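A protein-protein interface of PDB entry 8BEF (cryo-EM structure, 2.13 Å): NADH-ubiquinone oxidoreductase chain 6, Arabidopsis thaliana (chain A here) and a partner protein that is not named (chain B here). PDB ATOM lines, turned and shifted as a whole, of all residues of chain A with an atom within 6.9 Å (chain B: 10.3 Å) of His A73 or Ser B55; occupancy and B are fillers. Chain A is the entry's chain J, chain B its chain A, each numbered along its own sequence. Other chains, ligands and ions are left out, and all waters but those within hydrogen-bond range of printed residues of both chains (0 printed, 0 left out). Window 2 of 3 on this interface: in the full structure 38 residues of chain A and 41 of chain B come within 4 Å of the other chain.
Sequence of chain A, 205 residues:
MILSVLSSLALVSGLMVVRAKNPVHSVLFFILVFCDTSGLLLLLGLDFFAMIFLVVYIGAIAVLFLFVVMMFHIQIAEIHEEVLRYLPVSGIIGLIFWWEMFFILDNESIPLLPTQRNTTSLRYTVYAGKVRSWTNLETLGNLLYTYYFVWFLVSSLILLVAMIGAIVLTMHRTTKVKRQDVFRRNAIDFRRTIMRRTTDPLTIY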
ATOM      1  N   VAL A  68     -13.828   9.233 -28.061  1.00  0.00           N
ATOM      2  CA  VAL A  68     -14.432  10.437 -28.623  1.00  0.00           C
ATOM      3  C   VAL A  68     -15.955  10.347 -28.587  1.00  0.00           C
ATOM      4  O   VAL A  68     -16.635  11.274 -28.133  1.00  0.00           O
ATOM      5  CB  VAL A  68     -13.910  10.689 -30.047  1.00  0.00           C
ATOM      6  CG1 VAL A  68     -14.772  11.722 -30.750  1.00  0.00           C
ATOM      7  CG2 VAL A  68     -12.464  11.148 -29.994  1.00  0.00           C
ATOM      8  N   VAL A  69     -16.518   9.210 -29.018  1.00  0.00           N
ATOM      9  CA  VAL A  69     -17.993   9.061 -29.137  1.00  0.00           C
ATOM     10  C   VAL A  69     -18.639   9.045 -27.744  1.00  0.00           C
ATOM     11  O   VAL A  69     -19.574   9.764 -27.556  1.00  0.00           O
ATOM     12  CB  VAL A  69     -18.389   7.859 -30.027  1.00  0.00           C
ATOM     13  CG1 VAL A  69     -19.861   7.501 -29.988  1.00  0.00           C
ATOM     14  CG2 VAL A  69     -17.901   8.010 -31.458  1.00  0.00           C
ATOM     15  N   MET A  70     -17.971   8.479 -26.787  1.00  0.00           N
ATOM     16  CA  MET A  70     -18.541   8.403 -25.447  1.00  0.00           C
ATOM     17  C   MET A  70     -18.615   9.780 -24.798  1.00  0.00           C
ATOM     18  O   MET A  70     -19.611  10.113 -24.148  1.00  0.00           O
ATOM     19  CB  MET A  70     -17.708   7.448 -24.595  1.00  0.00           C
ATOM     20  CG  MET A  70     -18.167   6.005 -24.676  1.00  0.00           C
ATOM     21  SD  MET A  70     -17.229   4.915 -23.599  1.00  0.00           S
ATOM     22  CE  MET A  70     -18.023   3.347 -23.951  1.00  0.00           C
ATOM     23  N   MET A  71     -17.570  10.595 -24.962  1.00  0.00           N
ATOM     24  CA  MET A  71     -17.571  11.928 -24.372  1.00  0.00           C
ATOM     25  C   MET A  71     -18.462  12.902 -25.136  1.00  0.00           C
ATOM     26  O   MET A  71     -18.808  13.954 -24.593  1.00  0.00           O
ATOM     27  CB  MET A  71     -16.145  12.477 -24.296  1.00  0.00           C
ATOM     28  CG  MET A  71     -15.230  11.723 -23.346  1.00  0.00           C
ATOM     29  SD  MET A  71     -13.634  12.530 -23.120  1.00  0.00           S
ATOM     30  CE  MET A  71     -12.983  12.470 -24.784  1.00  0.00           C
ATOM     31  N   PHE A  72     -18.839  12.578 -26.377  1.00  0.00           N
ATOM     32  CA  PHE A  72     -19.747  13.439 -27.130  1.00  0.00           C
ATOM     33  C   PHE A  72     -21.150  13.439 -26.534  1.00  0.00           C
ATOM     34  O   PHE A  72     -21.836  14.465 -26.583  1.00  0.00           O
ATOM     35  CB  PHE A  72     -19.811  12.999 -28.597  1.00  0.00           C
ATOM     36  CG  PHE A  72     -18.763  13.629 -29.482  1.00  0.00           C
ATOM     37  CD1 PHE A  72     -17.980  14.674 -29.030  1.00  0.00           C
ATOM     38  CD2 PHE A  72     -18.566  13.161 -30.774  1.00  0.00           C
ATOM     39  CE1 PHE A  72     -17.017  15.245 -29.846  1.00  0.00           C
ATOM     40  CE2 PHE A  72     -17.607  13.725 -31.597  1.00  0.00           C
ATOM     41  CZ  PHE A  72     -16.829  14.770 -31.130  1.00  0.00           C
ATOM     42  N   HIS A  73     -21.590  12.308 -25.974  1.00  0.00           N
ATOM     43  CA  HIS A  73     -22.939  12.160 -25.421  1.00  0.00           C
ATOM     44  C   HIS A  73     -24.002  12.585 -26.434  1.00  0.00           C
ATOM     45  O   HIS A  73     -24.842  13.445 -26.170  1.00  0.00           O
ATOM     46  CB  HIS A  73     -23.087  12.937 -24.112  1.00  0.00           C
ATOM     47  CG  HIS A  73     -22.217  12.426 -23.006  1.00  0.00           C
ATOM     48  ND1 HIS A  73     -21.038  13.039 -22.640  1.00  0.00           N
ATOM     49  CD2 HIS A  73     -22.354  11.357 -22.187  1.00  0.00           C
ATOM     50  CE1 HIS A  73     -20.485  12.368 -21.647  1.00  0.00           C
ATOM     51  NE2 HIS A  73     -21.265  11.345 -21.349  1.00  0.00           N
ATOM     52  N   ILE A  74     -23.920  11.984 -27.598  1.00  0.00           N
ATOM     53  CA  ILE A  74     -24.870  12.336 -28.688  1.00  0.00           C
ATOM     54  C   ILE A  74     -26.306  11.953 -28.332  1.00  0.00           C
ATOM     55  O   ILE A  74     -26.525  10.865 -27.873  1.00  0.00           O
ATOM     56  CB  ILE A  74     -24.445  11.760 -30.056  1.00  0.00           C
ATOM     57  CG1 ILE A  74     -23.108  12.369 -30.484  1.00  0.00           C
ATOM     58  CG2 ILE A  74     -25.511  11.944 -31.109  1.00  0.00           C
ATOM     59  CD1 ILE A  74     -22.123  11.372 -31.015  1.00  0.00           C
ATOM     60  N   GLN A  75     -27.204  12.893 -28.511  1.00  0.00           N
ATOM     61  CA  GLN A  75     -28.624  12.605 -28.385  1.00  0.00           C
ATOM     62  C   GLN A  75     -29.160  12.090 -29.714  1.00  0.00           C
ATOM     63  O   GLN A  75     -28.770  12.571 -30.782  1.00  0.00           O
ATOM     64  CB  GLN A  75     -29.394  13.851 -27.950  1.00  0.00           C
ATOM     65  CG  GLN A  75     -28.871  14.472 -26.666  1.00  0.00           C
ATOM     66  CD  GLN A  75     -28.584  13.436 -25.598  1.00  0.00           C
ATOM     67  OE1 GLN A  75     -29.500  12.876 -24.997  1.00  0.00           O
ATOM     68  NE2 GLN A  75     -27.305  13.174 -25.358  1.00  0.00           N
ATOM     69  N   ILE A  76     -30.058  11.106 -29.640  1.00  0.00           N
ATOM     70  CA  ILE A  76     -30.533  10.446 -30.851  1.00  0.00           C
ATOM     71  C   ILE A  76     -31.296  11.406 -31.751  1.00  0.00           C
ATOM     72  O   ILE A  76     -31.308  11.237 -32.975  1.00  0.00           O
ATOM     73  CB  ILE A  76     -31.379   9.209 -30.497  1.00  0.00           C
ATOM     74  CG1 ILE A  76     -31.666   8.413 -31.765  1.00  0.00           C
ATOM     75  CG2 ILE A  76     -32.682   9.619 -29.829  1.00  0.00           C
ATOM     76  CD1 ILE A  76     -30.512   7.574 -32.195  1.00  0.00           C
ATOM     77  N   GLU A  78     -30.485  14.262 -32.676  1.00  0.00           N
ATOM     78  CA  GLU A  78     -29.573  14.972 -33.560  1.00  0.00           C
ATOM     79  C   GLU A  78     -29.130  14.129 -34.750  1.00  0.00           C
ATOM     80  O   GLU A  78     -28.699  14.692 -35.761  1.00  0.00           O
ATOM     81  CB  GLU A  78     -28.358  15.447 -32.767  1.00  0.00           C
ATOM     82  CG  GLU A  78     -28.593  16.759 -32.032  1.00  0.00           C
ATOM     83  CD  GLU A  78     -27.558  17.026 -30.960  1.00  0.00           C
ATOM     84  OE1 GLU A  78     -26.846  16.078 -30.567  1.00  0.00           O
ATOM     85  OE2 GLU A  78     -27.456  18.186 -30.506  1.00  0.00           O
ATOM     86  N   SER B  55     -21.307  14.842 -20.118  1.00  0.00           N
ATOM     87  CA  SER B  55     -21.513  16.028 -20.937  1.00  0.00           C
ATOM     88  C   SER B  55     -20.389  17.037 -20.723  1.00  0.00           C
ATOM     89  O   SER B  55     -20.600  18.246 -20.818  1.00  0.00           O
ATOM     90  CB  SER B  55     -22.866  16.666 -20.619  1.00  0.00           C
ATOM     91  OG  SER B  55     -22.869  17.238 -19.323  1.00  0.00           O
ATOM     92  N   ARG B  56     -19.191  16.528 -20.435  1.00  0.00           N
ATOM     93  CA  ARG B  56     -18.021  17.345 -20.107  1.00  0.00           C
ATOM     94  C   ARG B  56     -16.840  16.816 -20.921  1.00  0.00           C
ATOM     95  O   ARG B  56     -16.100  15.944 -20.459  1.00  0.00           O
ATOM     96  CB  ARG B  56     -17.744  17.298 -18.612  1.00  0.00           C
ATOM     97  CG  ARG B  56     -18.893  17.799 -17.749  1.00  0.00           C
ATOM     98  CD  ARG B  56     -18.571  17.682 -16.271  1.00  0.00           C
ATOM     99  NE  ARG B  56     -18.415  16.292 -15.860  1.00  0.00           N
ATOM    100  CZ  ARG B  56     -19.420  15.489 -15.540  1.00  0.00           C
ATOM    101  NH1 ARG B  56     -20.677  15.900 -15.588  1.00  0.00           N
ATOM    102  NH2 ARG B  56     -19.158  14.240 -15.163  1.00  0.00           N
ATOM    103  N   PHE B  57     -16.656  17.348 -22.125  1.00  0.00           N
ATOM    104  CA  PHE B  57     -15.651  16.811 -23.034  1.00  0.00           C
ATOM    105  C   PHE B  57     -14.261  17.290 -22.631  1.00  0.00           C
ATOM    106  O   PHE B  57     -13.997  18.495 -22.595  1.00  0.00           O
ATOM    107  CB  PHE B  57     -15.962  17.219 -24.472  1.00  0.00           C
ATOM    108  CG  PHE B  57     -15.169  16.460 -25.500  1.00  0.00           C
ATOM    109  CD1 PHE B  57     -13.845  16.782 -25.757  1.00  0.00           C
ATOM    110  CD2 PHE B  57     -15.744  15.416 -26.197  1.00  0.00           C
ATOM    111  CE1 PHE B  57     -13.115  16.080 -26.695  1.00  0.00           C
ATOM    112  CE2 PHE B  57     -15.018  14.709 -27.136  1.00  0.00           C
ATOM    113  CZ  PHE B  57     -13.703  15.040 -27.383  1.00  0.00           C
ATOM    114  N   ASP B  58     -13.369  16.344 -22.347  1.00  0.00           N
ATOM    115  CA  ASP B  58     -11.992  16.644 -21.970  1.00  0.00           C
ATOM    116  C   ASP B  58     -11.092  16.186 -23.115  1.00  0.00           C
ATOM    117  O   ASP B  58     -10.951  14.984 -23.360  1.00  0.00           O
ATOM    118  CB  ASP B  58     -11.631  15.964 -20.650  1.00  0.00           C
ATOM    119  CG  ASP B  58     -10.194  16.222 -20.220  1.00  0.00           C
ATOM    120  OD1 ASP B  58      -9.457  16.939 -20.925  1.00  0.00           O
ATOM    121  OD2 ASP B  58      -9.800  15.701 -19.158  1.00  0.00           O
ATOM    122  N   PHE B  61      -8.056  13.285 -23.170  1.00  0.00           N
ATOM    123  CA  PHE B  61      -8.255  11.867 -23.452  1.00  0.00           C
ATOM    124  C   PHE B  61      -8.097  11.575 -24.940  1.00  0.00           C
ATOM    125  O   PHE B  61      -7.494  10.565 -25.320  1.00  0.00           O
ATOM    126  CB  PHE B  61      -9.625  11.426 -22.946  1.00  0.00           C
ATOM    127  CG  PHE B  61      -9.726  11.389 -21.450  1.00  0.00           C
ATOM    128  CD1 PHE B  61      -9.000  10.466 -20.716  1.00  0.00           C
ATOM    129  CD2 PHE B  61     -10.526  12.294 -20.774  1.00  0.00           C
ATOM    130  CE1 PHE B  61      -9.083  10.434 -19.335  1.00  0.00           C
ATOM    131  CE2 PHE B  61     -10.612  12.268 -19.395  1.00  0.00           C
ATOM    132  CZ  PHE B  61      -9.889  11.338 -18.675  1.00  0.00           C
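Of the 5 printed residues of chain B, 4 touch a printed residue of chain A. Of the 10 printed residues of chain A, 4 touch a printed residue of chain B. Among the printed residues, no Asp or Glu carboxylate lies within 4 Å of a Lys or Arg side-chain nitrogen of the other chain.
N of Ser B55 sits close to ND1 of His A73 (3.1 Å). The side-chain sulfur of Met A71 lies close to the backbone carbonyl oxygen of Asp B58 (3.6 Å).
CE2 of Phe B57 touches O of Val A68, at 3.9 Å. Met A71 touches Phe B57. SD of Met A71 touches CD2 of Phe B61, at 3.9 Å. Phe B57 touches Phe A72 (CE2 to CE1, 3.4 Å).
Of chain B, only Ser B55 comes within 4 Å of His A73. Ser B55 touches one residue of chain A. No residue of chain B comes within 4 Å of Ile A74. No residue of chain B comes within 4 Å of Gln A75. Printed residues of chain B within 4 Å of Met A71: Phe B57 (3.5 Å), Asp B58 (3.5 Å) and Phe B61 (3.9 Å). Printed residues of chain A within 4 Å of Asp B58: Met A71. Printed residues of chain A within 4 Å of Phe B61: Met A71. Printed residues of chain B within 4 Å of Val A68: Phe B57. Of the printed residues of chain B, Phe A72 touches Phe B57. Met A70 touches none of the printed residues of chain B. Glu A78 touches none of the printed residues of chain B. The nearest residue of chain A that does not touch Ser B55 is Met A71 (5.0 Å). The nearest printed residue of chain A that does not touch Phe B57 is Val A69 (6.0 Å).
A ring nitrogen (NE2) of His A73 sits at hydrogen-bond distance from the backbone carbonyl oxygen of Met A70 (3.5 Å). A ring nitrogen (ND1) of His A73 is in hydrogen-bond range of the backbone carbonyl oxygen (O) of Met A71, 3.1 Å away. The side-chain amide nitrogen (NE2) of Gln A75 lies within hydrogen-bond range of the backbone carbonyl oxygen (O) of His A73, at 2.6 Å.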
